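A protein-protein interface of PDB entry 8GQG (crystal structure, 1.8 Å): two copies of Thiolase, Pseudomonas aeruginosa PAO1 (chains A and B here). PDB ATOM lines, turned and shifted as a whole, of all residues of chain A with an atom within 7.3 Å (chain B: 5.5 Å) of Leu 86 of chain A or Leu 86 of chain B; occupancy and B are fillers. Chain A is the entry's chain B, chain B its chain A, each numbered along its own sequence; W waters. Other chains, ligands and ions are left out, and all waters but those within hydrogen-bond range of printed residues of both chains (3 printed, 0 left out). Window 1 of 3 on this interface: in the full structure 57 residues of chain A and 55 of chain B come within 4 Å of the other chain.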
ATOM      1  N   ILE A  53      31.088  14.437  14.821  1.00  0.00           N
ATOM      2  CA  ILE A  53      30.689  13.028  15.020  1.00  0.00           C
ATOM      3  C   ILE A  53      29.906  12.965  16.305  1.00  0.00           C
ATOM      4  O   ILE A  53      30.488  13.214  17.355  1.00  0.00           O
ATOM      5  CB  ILE A  53      31.908  12.100  15.037  1.00  0.00           C
ATOM      6  CG1 ILE A  53      32.806  12.359  13.823  1.00  0.00           C
ATOM      7  CG2 ILE A  53      31.442  10.663  15.092  1.00  0.00           C
ATOM      8  CD1 ILE A  53      34.118  11.616  13.855  1.00  0.00           C
ATOM      9  N   VAL A  54      28.638  12.572  16.197  1.00  0.00           N
ATOM     10  CA  VAL A  54      27.702  12.520  17.340  1.00  0.00           C
ATOM     11  C   VAL A  54      27.163  11.095  17.505  1.00  0.00           C
ATOM     12  O   VAL A  54      26.534  10.568  16.566  1.00  0.00           O
ATOM     13  CB  VAL A  54      26.588  13.560  17.115  1.00  0.00           C
ATOM     14  CG1 VAL A  54      25.531  13.468  18.182  1.00  0.00           C
ATOM     15  CG2 VAL A  54      27.169  14.955  17.029  1.00  0.00           C
ATOM     16  N   GLY A  55      27.448  10.497  18.659  1.00  0.00           N
ATOM     17  CA  GLY A  55      26.883   9.218  19.098  1.00  0.00           C
ATOM     18  C   GLY A  55      25.557   9.452  19.825  1.00  0.00           C
ATOM     19  O   GLY A  55      25.428  10.432  20.587  1.00  0.00           O
ATOM     20  N   ALA A  56      24.617   8.529  19.617  1.00  0.00           N
ATOM     21  CA  ALA A  56      23.283   8.544  20.239  1.00  0.00           C
ATOM     22  C   ALA A  56      22.708   7.134  20.170  1.00  0.00           C
ATOM     23  O   ALA A  56      22.912   6.463  19.099  1.00  0.00           O
ATOM     24  CB  ALA A  56      22.443   9.515  19.455  1.00  0.00           C
ATOM     25  N   GLY A  57      22.026   6.717  21.239  1.00  0.00           N
ATOM     26  CA  GLY A  57      21.357   5.419  21.335  1.00  0.00           C
ATOM     27  C   GLY A  57      20.183   5.387  20.388  1.00  0.00           C
ATOM     28  O   GLY A  57      20.157   4.528  19.476  1.00  0.00           O
ATOM     29  N   SER A  58      19.250   6.341  20.549  1.00  0.00           N
ATOM     30  CA  SER A  58      18.114   6.453  19.615  1.00  0.00           C
ATOM     31  C   SER A  58      18.632   7.204  18.394  1.00  0.00           C
ATOM     32  O   SER A  58      19.342   8.199  18.596  1.00  0.00           O
ATOM     33  CB  SER A  58      16.915   7.138  20.254  1.00  0.00           C
ATOM     34  OG  SER A  58      15.982   7.485  19.237  1.00  0.00           O
ATOM     35  N   ASN A  59      18.312   6.745  17.197  1.00  0.00           N
ATOM     36  CA  ASN A  59      18.683   7.446  15.941  1.00  0.00           C
ATOM     37  C   ASN A  59      17.442   7.756  15.111  1.00  0.00           C
ATOM     38  O   ASN A  59      17.499   7.717  13.857  1.00  0.00           O
ATOM     39  CB  ASN A  59      19.695   6.640  15.137  1.00  0.00           C
ATOM     40  CG  ASN A  59      21.006   6.379  15.859  1.00  0.00           C
ATOM     41  OD1 ASN A  59      21.443   7.133  16.753  1.00  0.00           O
ATOM     42  ND2 ASN A  59      21.644   5.317  15.440  1.00  0.00           N
ATOM     43  N   ASN A  66      20.108  12.251  10.671  1.00  0.00           N
ATOM     44  CA  ASN A  66      21.592  12.445  10.799  1.00  0.00           C
ATOM     45  C   ASN A  66      21.865  13.626  11.735  1.00  0.00           C
ATOM     46  O   ASN A  66      22.321  14.724  11.292  1.00  0.00           O
ATOM     47  CB  ASN A  66      22.325  12.560   9.463  1.00  0.00           C
ATOM     48  CG  ASN A  66      23.840  12.588   9.635  1.00  0.00           C
ATOM     49  OD1 ASN A  66      24.376  12.400  10.738  1.00  0.00           O
ATOM     50  ND2 ASN A  66      24.527  12.905   8.559  1.00  0.00           N
ATOM     51  N   ILE A  67      21.627  13.387  13.012  1.00  0.00           N
ATOM     52  CA  ILE A  67      21.817  14.393  14.086  1.00  0.00           C
ATOM     53  C   ILE A  67      23.243  14.978  14.023  1.00  0.00           C
ATOM     54  O   ILE A  67      23.385  16.198  14.203  1.00  0.00           O
ATOM     55  CB  ILE A  67      21.410  13.812  15.450  1.00  0.00           C
ATOM     56  CG1 ILE A  67      21.533  14.883  16.533  1.00  0.00           C
ATOM     57  CG2 ILE A  67      22.151  12.537  15.814  1.00  0.00           C
ATOM     58  CD1 ILE A  67      20.804  14.554  17.803  1.00  0.00           C
ATOM     59  N   GLY A  68      24.287  14.188  13.756  1.00  0.00           N
ATOM     60  CA  GLY A  68      25.662  14.739  13.705  1.00  0.00           C
ATOM     61  C   GLY A  68      25.855  15.857  12.675  1.00  0.00           C
ATOM     62  O   GLY A  68      26.478  16.886  13.015  1.00  0.00           O
ATOM     63  N   MET A  84      28.171  13.235  11.052  1.00  0.00           N
ATOM     64  CA  MET A  84      27.656  11.851  10.965  1.00  0.00           C
ATOM     65  C   MET A  84      27.148  11.453  12.344  1.00  0.00           C
ATOM     66  O   MET A  84      27.528  12.084  13.370  1.00  0.00           O
ATOM     67  CB  MET A  84      28.701  10.842  10.469  1.00  0.00           C
ATOM     68  CG  MET A  84      29.869  10.722  11.371  1.00  0.00           C
ATOM     69  SD  MET A  84      30.987   9.297  11.041  1.00  0.00           S
ATOM     70  CE  MET A  84      30.168   8.055  12.043  1.00  0.00           C
ATOM     71  N   THR A  85      26.353  10.386  12.345  1.00  0.00           N
ATOM     72  CA  THR A  85      25.749   9.815  13.562  1.00  0.00           C
ATOM     73  C   THR A  85      26.247   8.379  13.715  1.00  0.00           C
ATOM     74  O   THR A  85      26.464   7.699  12.714  1.00  0.00           O
ATOM     75  CB  THR A  85      24.225   9.869  13.425  1.00  0.00           C
ATOM     76  OG1 THR A  85      23.833  11.223  13.147  1.00  0.00           O
ATOM     77  CG2 THR A  85      23.547   9.338  14.662  1.00  0.00           C
ATOM     78  N   LEU A  86      26.362   7.892  14.929  1.00  0.00           N
ATOM     79  CA  LEU A  86      26.600   6.449  15.122  1.00  0.00           C
ATOM     80  C   LEU A  86      25.890   6.006  16.397  1.00  0.00           C
ATOM     81  O   LEU A  86      25.585   6.828  17.255  1.00  0.00           O
ATOM     82  CB  LEU A  86      28.112   6.185  15.168  1.00  0.00           C
ATOM     83  CG  LEU A  86      28.808   6.851  16.353  1.00  0.00           C
ATOM     84  CD1 LEU A  86      28.787   5.969  17.596  1.00  0.00           C
ATOM     85  CD2 LEU A  86      30.232   7.245  16.034  1.00  0.00           C
ATOM     86  N   ASN A  87      25.684   4.706  16.473  1.00  0.00           N
ATOM     87  CA  ASN A  87      25.062   3.967  17.596  1.00  0.00           C
ATOM     88  C   ASN A  87      25.913   2.739  17.893  1.00  0.00           C
ATOM     89  O   ASN A  87      25.910   1.808  17.094  1.00  0.00           O
ATOM     90  CB  ASN A  87      23.628   3.576  17.238  1.00  0.00           C
ATOM     91  CG  ASN A  87      22.907   2.832  18.347  1.00  0.00           C
ATOM     92  OD1 ASN A  87      23.359   2.785  19.476  1.00  0.00           O
ATOM     93  ND2 ASN A  87      21.812   2.160  18.009  1.00  0.00           N
ATOM     94  N   ARG A  88      26.582   2.733  19.048  1.00  0.00           N
ATOM     95  CA  ARG A  88      26.970   1.519  19.789  1.00  0.00           C
ATOM     96  C   ARG A  88      26.452   1.714  21.213  1.00  0.00           C
ATOM     97  O   ARG A  88      27.252   1.673  22.121  1.00  0.00           O
ATOM     98  CB  ARG A  88      28.488   1.276  19.722  1.00  0.00           C
ATOM     99  CG  ARG A  88      28.805  -0.192  19.939  1.00  0.00           C
ATOM    100  CD  ARG A  88      30.261  -0.482  20.151  1.00  0.00           C
ATOM    101  NE  ARG A  88      31.145  -0.162  19.055  1.00  0.00           N
ATOM    102  CZ  ARG A  88      31.561  -1.025  18.129  1.00  0.00           C
ATOM    103  NH1 ARG A  88      31.038  -2.233  18.023  1.00  0.00           N
ATOM    104  NH2 ARG A  88      32.465  -0.639  17.250  1.00  0.00           N
ATOM    105  N   TYR A  89      25.146   2.021  21.313  1.00  0.00           N
ATOM    106  CA  TYR A  89      24.334   2.401  22.510  1.00  0.00           C
ATOM    107  C   TYR A  89      25.192   3.152  23.566  1.00  0.00           C
ATOM    108  O   TYR A  89      25.673   4.282  23.306  1.00  0.00           O
ATOM    109  CB  TYR A  89      23.608   1.143  23.025  1.00  0.00           C
ATOM    110  CG  TYR A  89      22.384   0.669  22.262  1.00  0.00           C
ATOM    111  CD1 TYR A  89      21.309   1.505  22.005  1.00  0.00           C
ATOM    112  CD2 TYR A  89      22.264  -0.658  21.860  1.00  0.00           C
ATOM    113  CE1 TYR A  89      20.180   1.050  21.340  1.00  0.00           C
ATOM    114  CE2 TYR A  89      21.146  -1.135  21.190  1.00  0.00           C
ATOM    115  CZ  TYR A  89      20.112  -0.270  20.928  1.00  0.00           C
ATOM    116  OH  TYR A  89      19.013  -0.738  20.309  1.00  0.00           O
ATOM    117  N   SER A  91      28.167   3.074  24.578  1.00  0.00           N
ATOM    118  CA  SER A  91      29.581   3.425  24.285  1.00  0.00           C
ATOM    119  C   SER A  91      29.654   4.535  23.242  1.00  0.00           C
ATOM    120  O   SER A  91      30.788   4.976  22.934  1.00  0.00           O
ATOM    121  CB  SER A  91      30.340   2.198  23.855  1.00  0.00           C
ATOM    122  OG  SER A  91      29.928   1.784  22.558  1.00  0.00           O
ATOM    123  N   SER A  92      28.518   4.960  22.682  1.00  0.00           N
ATOM    124  CA  SER A  92      28.505   5.840  21.485  1.00  0.00           C
ATOM    125  C   SER A  92      29.396   7.072  21.621  1.00  0.00           C
ATOM    126  O   SER A  92      30.049   7.421  20.607  1.00  0.00           O
ATOM    127  CB  SER A  92      27.112   6.214  21.061  1.00  0.00           C
ATOM    128  OG  SER A  92      26.321   5.055  20.922  1.00  0.00           O
ATOM    129  N   GLY A  93      29.403   7.770  22.755  1.00  0.00           N
ATOM    130  CA  GLY A  93      30.203   8.994  22.883  1.00  0.00           C
ATOM    131  C   GLY A  93      31.690   8.699  22.833  1.00  0.00           C
ATOM    132  O   GLY A  93      32.437   9.535  22.307  1.00  0.00           O
ATOM    133  N   LEU A  94      32.118   7.589  23.437  1.00  0.00           N
ATOM    134  CA  LEU A  94      33.541   7.175  23.367  1.00  0.00           C
ATOM    135  C   LEU A  94      33.880   6.728  21.939  1.00  0.00           C
ATOM    136  O   LEU A  94      34.987   7.102  21.403  1.00  0.00           O
ATOM    137  CB  LEU A  94      33.792   6.073  24.388  1.00  0.00           C
ATOM    138  CG  LEU A  94      35.187   5.437  24.363  1.00  0.00           C
ATOM    139  CD1 LEU A  94      36.294   6.440  24.678  1.00  0.00           C
ATOM    140  CD2 LEU A  94      35.228   4.282  25.331  1.00  0.00           C
ATOM    141  N   GLN A  95      33.002   5.923  21.353  1.00  0.00           N
ATOM    142  CA  GLN A  95      33.169   5.417  19.978  1.00  0.00           C
ATOM    143  C   GLN A  95      33.383   6.610  19.036  1.00  0.00           C
ATOM    144  O   GLN A  95      34.258   6.509  18.121  1.00  0.00           O
ATOM    145  CB  GLN A  95      31.950   4.594  19.558  1.00  0.00           C
ATOM    146  CG  GLN A  95      32.052   4.053  18.142  1.00  0.00           C
ATOM    147  CD  GLN A  95      33.139   2.994  18.048  1.00  0.00           C
ATOM    148  OE1 GLN A  95      32.993   1.861  18.497  1.00  0.00           O
ATOM    149  NE2 GLN A  95      34.255   3.366  17.451  1.00  0.00           N
ATOM    150  N   ALA A  96      32.625   7.694  19.213  1.00  0.00           N
ATOM    151  CA  ALA A  96      32.721   8.900  18.363  1.00  0.00           C
ATOM    152  C   ALA A  96      34.139   9.475  18.500  1.00  0.00           C
ATOM    153  O   ALA A  96      34.754   9.884  17.500  1.00  0.00           O
ATOM    154  CB  ALA A  96      31.697   9.917  18.747  1.00  0.00           C
ATOM    155  N   ILE A  97      34.610   9.559  19.717  1.00  0.00           N
ATOM    156  CA  ILE A  97      35.945  10.148  20.007  1.00  0.00           C
ATOM    157  C   ILE A  97      37.052   9.272  19.377  1.00  0.00           C
ATOM    158  O   ILE A  97      37.987   9.835  18.749  1.00  0.00           O
ATOM    159  CB  ILE A  97      36.080  10.330  21.529  1.00  0.00           C
ATOM    160  CG1 ILE A  97      35.176  11.480  22.017  1.00  0.00           C
ATOM    161  CG2 ILE A  97      37.525  10.505  21.924  1.00  0.00           C
ATOM    162  CD1 ILE A  97      35.023  11.527  23.512  1.00  0.00           C
ATOM    163  N   ILE A  99      36.786   7.303  16.753  1.00  0.00           N
ATOM    164  CA  ILE A  99      36.698   7.456  15.281  1.00  0.00           C
ATOM    165  C   ILE A  99      37.363   8.769  14.884  1.00  0.00           C
ATOM    166  O   ILE A  99      38.168   8.747  13.937  1.00  0.00           O
ATOM    167  CB  ILE A  99      35.240   7.364  14.811  1.00  0.00           C
ATOM    168  CG1 ILE A  99      34.744   5.921  14.854  1.00  0.00           C
ATOM    169  CG2 ILE A  99      35.109   7.985  13.431  1.00  0.00           C
ATOM    170  CD1 ILE A  99      33.224   5.769  14.823  1.00  0.00           C
ATOM    171  N   GLY A 115      31.487  13.448  20.084  1.00  0.00           N
ATOM    172  CA  GLY A 115      30.912  13.161  21.389  1.00  0.00           C
ATOM    173  C   GLY A 115      29.548  12.540  21.196  1.00  0.00           C
ATOM    174  O   GLY A 115      29.389  11.741  20.226  1.00  0.00           O
ATOM    175  N   GLY A 352      24.039   8.037  24.754  1.00  0.00           N
ATOM    176  CA  GLY A 352      24.949   8.628  23.754  1.00  0.00           C
ATOM    177  C   GLY A 352      26.053   9.476  24.352  1.00  0.00           C
ATOM    178  O   GLY A 352      27.163   9.535  23.772  1.00  0.00           O
ATOM    179  N   ILE B  53      30.753  -3.470  11.369  1.00  0.00           N
ATOM    180  CA  ILE B  53      30.344  -2.058  11.218  1.00  0.00           C
ATOM    181  C   ILE B  53      29.363  -1.965  10.062  1.00  0.00           C
ATOM    182  O   ILE B  53      29.756  -2.279   8.906  1.00  0.00           O
ATOM    183  CB  ILE B  53      31.546  -1.140  10.991  1.00  0.00           C
ATOM    184  CG1 ILE B  53      32.621  -1.409  12.038  1.00  0.00           C
ATOM    185  CG2 ILE B  53      31.092   0.304  11.010  1.00  0.00           C
ATOM    186  CD1 ILE B  53      33.869  -0.535  11.852  1.00  0.00           C
ATOM    187  N   VAL B  54      28.120  -1.605  10.388  1.00  0.00           N
ATOM    188  CA  VAL B  54      27.057  -1.484   9.357  1.00  0.00           C
ATOM    189  C   VAL B  54      26.559  -0.048   9.224  1.00  0.00           C
ATOM    190  O   VAL B  54      26.008   0.497  10.189  1.00  0.00           O
ATOM    191  CB  VAL B  54      25.951  -2.492   9.649  1.00  0.00           C
ATOM    192  CG1 VAL B  54      24.822  -2.354   8.656  1.00  0.00           C
ATOM    193  CG2 VAL B  54      26.540  -3.896   9.640  1.00  0.00           C
ATOM    194  N   GLY B  55      26.701   0.500   8.022  1.00  0.00           N
ATOM    195  CA  GLY B  55      26.144   1.793   7.627  1.00  0.00           C
ATOM    196  C   GLY B  55      24.731   1.606   7.094  1.00  0.00           C
ATOM    197  O   GLY B  55      24.438   0.612   6.381  1.00  0.00           O
ATOM    198  N   ALA B  56      23.857   2.529   7.424  1.00  0.00           N
ATOM    199  CA  ALA B  56      22.465   2.523   6.948  1.00  0.00           C
ATOM    200  C   ALA B  56      21.919   3.955   7.077  1.00  0.00           C
ATOM    201  O   ALA B  56      22.300   4.657   8.032  1.00  0.00           O
ATOM    202  CB  ALA B  56      21.685   1.513   7.759  1.00  0.00           C
ATOM    203  N   GLY B  57      21.129   4.381   6.095  1.00  0.00           N
ATOM    204  CA  GLY B  57      20.451   5.692   6.079  1.00  0.00           C
ATOM    205  C   GLY B  57      19.343   5.738   7.122  1.00  0.00           C
ATOM    206  O   GLY B  57      19.445   6.535   8.066  1.00  0.00           O
ATOM    207  N   ASN B  59      17.893   4.297  10.476  1.00  0.00           N
ATOM    208  CA  ASN B  59      18.423   3.582  11.651  1.00  0.00           C
ATOM    209  C   ASN B  59      17.269   3.256  12.612  1.00  0.00           C
ATOM    210  O   ASN B  59      17.471   3.323  13.832  1.00  0.00           O
ATOM    211  CB  ASN B  59      19.529   4.391  12.321  1.00  0.00           C
ATOM    212  CG  ASN B  59      20.734   4.635  11.440  1.00  0.00           C
ATOM    213  OD1 ASN B  59      21.000   3.948  10.417  1.00  0.00           O
ATOM    214  ND2 ASN B  59      21.503   5.602  11.872  1.00  0.00           N
ATOM    215  N   MET B  84      28.367  -2.172  15.442  1.00  0.00           N
ATOM    216  CA  MET B  84      27.841  -0.798  15.589  1.00  0.00           C
ATOM    217  C   MET B  84      27.179  -0.433  14.277  1.00  0.00           C
ATOM    218  O   MET B  84      27.437  -1.098  13.226  1.00  0.00           O
ATOM    219  CB  MET B  84      28.935   0.208  15.915  1.00  0.00           C
ATOM    220  CG  MET B  84      30.047   0.251  14.901  1.00  0.00           C
ATOM    221  SD  MET B  84      31.126   1.656  15.202  1.00  0.00           S
ATOM    222  CE  MET B  84      30.113   2.870  14.354  1.00  0.00           C
ATOM    223  N   THR B  85      26.393   0.627  14.360  1.00  0.00           N
ATOM    224  CA  THR B  85      25.619   1.223  13.271  1.00  0.00           C
ATOM    225  C   THR B  85      26.107   2.653  13.078  1.00  0.00           C
ATOM    226  O   THR B  85      26.554   3.313  14.072  1.00  0.00           O
ATOM    227  CB  THR B  85      24.120   1.152  13.600  1.00  0.00           C
ATOM    228  OG1 THR B  85      23.796  -0.211  13.914  1.00  0.00           O
ATOM    229  CG2 THR B  85      23.283   1.671  12.454  1.00  0.00           C
ATOM    230  N   LEU B  86      26.051   3.130  11.850  1.00  0.00           N
ATOM    231  CA  LEU B  86      26.335   4.572  11.616  1.00  0.00           C
ATOM    232  C   LEU B  86      25.487   5.082  10.461  1.00  0.00           C
ATOM    233  O   LEU B  86      25.006   4.286   9.627  1.00  0.00           O
ATOM    234  CB  LEU B  86      27.835   4.808  11.393  1.00  0.00           C
ATOM    235  CG  LEU B  86      28.482   4.180  10.155  1.00  0.00           C
ATOM    236  CD1 LEU B  86      28.300   5.046   8.942  1.00  0.00           C
ATOM    237  CD2 LEU B  86      29.982   3.997  10.403  1.00  0.00           C
ATOM    238  N   ASN B  87      25.381   6.401  10.400  1.00  0.00           N
ATOM    239  CA  ASN B  87      24.626   7.093   9.341  1.00  0.00           C
ATOM    240  C   ASN B  87      25.421   8.330   8.925  1.00  0.00           C
ATOM    241  O   ASN B  87      25.574   9.229   9.754  1.00  0.00           O
ATOM    242  CB  ASN B  87      23.239   7.458   9.860  1.00  0.00           C
ATOM    243  CG  ASN B  87      22.469   8.304   8.881  1.00  0.00           C
ATOM    244  OD1 ASN B  87      22.712   8.272   7.682  1.00  0.00           O
ATOM    245  ND2 ASN B  87      21.463   9.011   9.364  1.00  0.00           N
ATOM    246  N   ARG B  88      25.970   8.293   7.723  1.00  0.00           N
ATOM    247  CA  ARG B  88      26.303   9.474   6.919  1.00  0.00           C
ATOM    248  C   ARG B  88      25.602   9.257   5.568  1.00  0.00           C
ATOM    249  O   ARG B  88      26.267   9.371   4.538  1.00  0.00           O
ATOM    250  CB  ARG B  88      27.815   9.705   6.925  1.00  0.00           C
ATOM    251  CG  ARG B  88      28.137  11.136   6.513  1.00  0.00           C
ATOM    252  CD  ARG B  88      29.590  11.417   6.244  1.00  0.00           C
ATOM    253  NE  ARG B  88      30.579  11.109   7.267  1.00  0.00           N
ATOM    254  CZ  ARG B  88      31.097  11.989   8.113  1.00  0.00           C
ATOM    255  NH1 ARG B  88      30.664  13.248   8.193  1.00  0.00           N
ATOM    256  NH2 ARG B  88      32.083  11.608   8.893  1.00  0.00           N
ATOM    257  N   SER B  92      27.491   5.979   3.809  1.00  0.00           N
ATOM    258  CA  SER B  92      27.597   5.179   5.051  1.00  0.00           C
ATOM    259  C   SER B  92      28.442   3.932   4.824  1.00  0.00           C
ATOM    260  O   SER B  92      29.200   3.612   5.744  1.00  0.00           O
ATOM    261  CB  SER B  92      26.235   4.828   5.630  1.00  0.00           C
ATOM    262  OG  SER B  92      25.491   6.012   5.940  1.00  0.00           O
ATOM    263  N   GLN B  95      32.010   5.026   4.686  1.00  0.00           N
ATOM    264  CA  GLN B  95      32.338   5.548   6.043  1.00  0.00           C
ATOM    265  C   GLN B  95      32.664   4.373   6.970  1.00  0.00           C
ATOM    266  O   GLN B  95      33.678   4.418   7.770  1.00  0.00           O
ATOM    267  CB  GLN B  95      31.173   6.385   6.600  1.00  0.00           C
ATOM    268  CG  GLN B  95      31.434   6.905   8.001  1.00  0.00           C
ATOM    269  CD  GLN B  95      32.553   7.935   7.967  1.00  0.00           C
ATOM    270  OE1 GLN B  95      32.384   9.065   7.542  1.00  0.00           O
ATOM    271  NE2 GLN B  95      33.727   7.509   8.379  1.00  0.00           N
ATOM    272  N   ALA B  96      31.882   3.312   6.875  1.00  0.00           N
ATOM    273  CA  ALA B  96      32.122   2.112   7.709  1.00  0.00           C
ATOM    274  C   ALA B  96      33.508   1.498   7.432  1.00  0.00           C
ATOM    275  O   ALA B  96      34.206   1.108   8.371  1.00  0.00           O
ATOM    276  CB  ALA B  96      31.032   1.094   7.443  1.00  0.00           C
ATOM    277  N   ILE B  99      36.280   3.701   8.837  1.00  0.00           N
ATOM    278  CA  ILE B  99      36.406   3.518  10.302  1.00  0.00           C
ATOM    279  C   ILE B  99      37.154   2.207  10.562  1.00  0.00           C
ATOM    280  O   ILE B  99      38.010   2.170  11.478  1.00  0.00           O
ATOM    281  CB  ILE B  99      35.033   3.587  10.996  1.00  0.00           C
ATOM    282  CG1 ILE B  99      34.550   5.045  11.035  1.00  0.00           C
ATOM    283  CG2 ILE B  99      35.094   2.972  12.396  1.00  0.00           C
ATOM    284  CD1 ILE B  99      33.040   5.175  11.167  1.00  0.00           C
HETATM  285  O   HOH W   1      16.454   6.532  11.633  1.00  0.00           O
HETATM  286  O   HOH W   2      23.722   5.590  13.465  1.00  0.00           O
HETATM  287  O   HOH W   3      16.641   4.612  16.168  1.00  0.00           O
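SD of Met 84 of chain B sits at hydrogen-bond distance from NH2 of Arg 88 of chain A (3.4 Å).
The side-chain amide oxygen of Gln 95 of chain A lies close to the side-chain sulfur of Met 84 of chain B, at 3.8 Å.
O of Thr 85 of chain B is in hydrogen-bond range of N of Asn 87 of chain A (2.9 Å).
O of Thr 85 of chain A lies within hydrogen-bond range of N of Asn 87 of chain B (2.9 Å).
The side-chain sulfur of Met 84 of chain A sits at hydrogen-bond distance from the guanidinium group of Arg 88 of chain B (3.3 Å).
The side-chain amide oxygen (OE1) of Gln 95 of chain B sits close to the side-chain sulfur (SD) of Met 84 of chain A, at 3.8 Å.
NE of Arg 88 of chain B sits at hydrogen-bond distance from OE1 of Gln 95 of chain B (2.7 Å).
N of Val 54 of chain A is in hydrogen-bond range of O of Met 84 of chain A, at 3.1 Å.
The backbone carbonyl oxygen (O) of Ala 56 of chain A lies close to the side-chain amide oxygen (OD1) of Asn 59 of chain A, at 2.8 Å.
The backbone NH of Gly 68 of chain A lies within hydrogen-bond range of the side-chain hydroxyl of Thr 85 of chain A.
OD1 of Asn 87 of chain A lies within hydrogen-bond range of N of Tyr 89 of chain A (2.7 Å).
The guanidinium group (NE) of Arg 88 of chain A is in hydrogen-bond range of the side-chain amide oxygen (OE1) of Gln 95 of chain A, at 2.8 Å.
Among the printed residues, pairs that only touch across the chains: Leu 86 of chain A with Thr 85 of chain B (3.3 Å), Thr 85 of chain A with Leu 86 of chain B (3.3 Å), Asn 66 of chain A with Asn 87 of chain B (3.5 Å), Met 84 of chain A with Asn 87 of chain B (3.6 Å), Asn 87 of chain A with Met 84 of chain B (3.6 Å), Asn 59 of chain A with Asn 59 of chain B (3.6 Å), Ile 99 of chain A with Ile 99 of chain B (3.7 Å), Leu 86 of chain A with Met 84 of chain B (3.96 Å) and Leu 86 of chain A with Leu 86 of chain B (3.99 Å).
Printed residues of chain A within 4 Å of Leu 86 of chain B: Thr 85 (3.3 Å) and Leu 86 (3.99 Å).
Printed residues of chain A within 4 Å of Asn 87 of chain B: Asn 66 (3.5 Å), Met 84 (3.6 Å) and Thr 85 (2.9 Å).
Of the printed residues of chain B, Met 84 of chain A touches Asn 87, Arg 88 and Gln 95.
Of the printed residues of chain A, Ile 99 of chain B touches Ile 99.
Of the printed residues of chain B, Thr 85 of chain A touches Leu 86 (3.3 Å) and Asn 87 (2.9 Å).
Printed residues of chain B within 4 Å of Asn 66 of chain A: Asn 87 (3.5 Å).
The nearest printed residue of chain A that does not touch Leu 86 of chain B is Met 84 of chain A (4.1 Å).
Along chain A the printed residues that touch a printed residue of chain B span positions 59 to 99.
Of the 15 printed residues of chain B, 8 touch a printed residue of chain A.
Hydrophobic or aromatic side chains of chain B within 4 Å of the printed part of chain A: Met 84, Leu 86 and Ile 99.
Among the printed residues, 15 pairs touch across the chains.
Among the printed residues, no Asp or Glu carboxylate lies within 4 Å of a Lys or Arg side-chain nitrogen of the other chain.
Asn 59 of chain B touches its own counterpart, Asn 59 of chain A.
Met 84 of chain A touches Arg 88 of chain B, and with the chains exchanged Arg 88 of chain A touches Met 84 of chain B.
Met 84 of chain A touches Gln 95 of chain B, and with the chains exchanged Gln 95 of chain A touches Met 84 of chain B.
Thr 85 of chain A touches Asn 87 of chain B, and with the chains exchanged Asn 87 of chain A touches Thr 85 of chain B.
15 positions are printed for both chains.
Water W1 lies within hydrogen-bond range of the backbone carbonyl oxygen of Asn 59 of chain A and the backbone NH of Asn 59 of chain B.
Water W2 bridges the side-chain amide nitrogen (ND2) of Asn 59 of chain B and the side-chain amide nitrogen (ND2) of Asn 59 of chain A.
Water W3 lies within hydrogen-bond range of O of Asn 59 of chain B (2.8 Å) and N of Asn 59 of chain A (2.9 Å).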
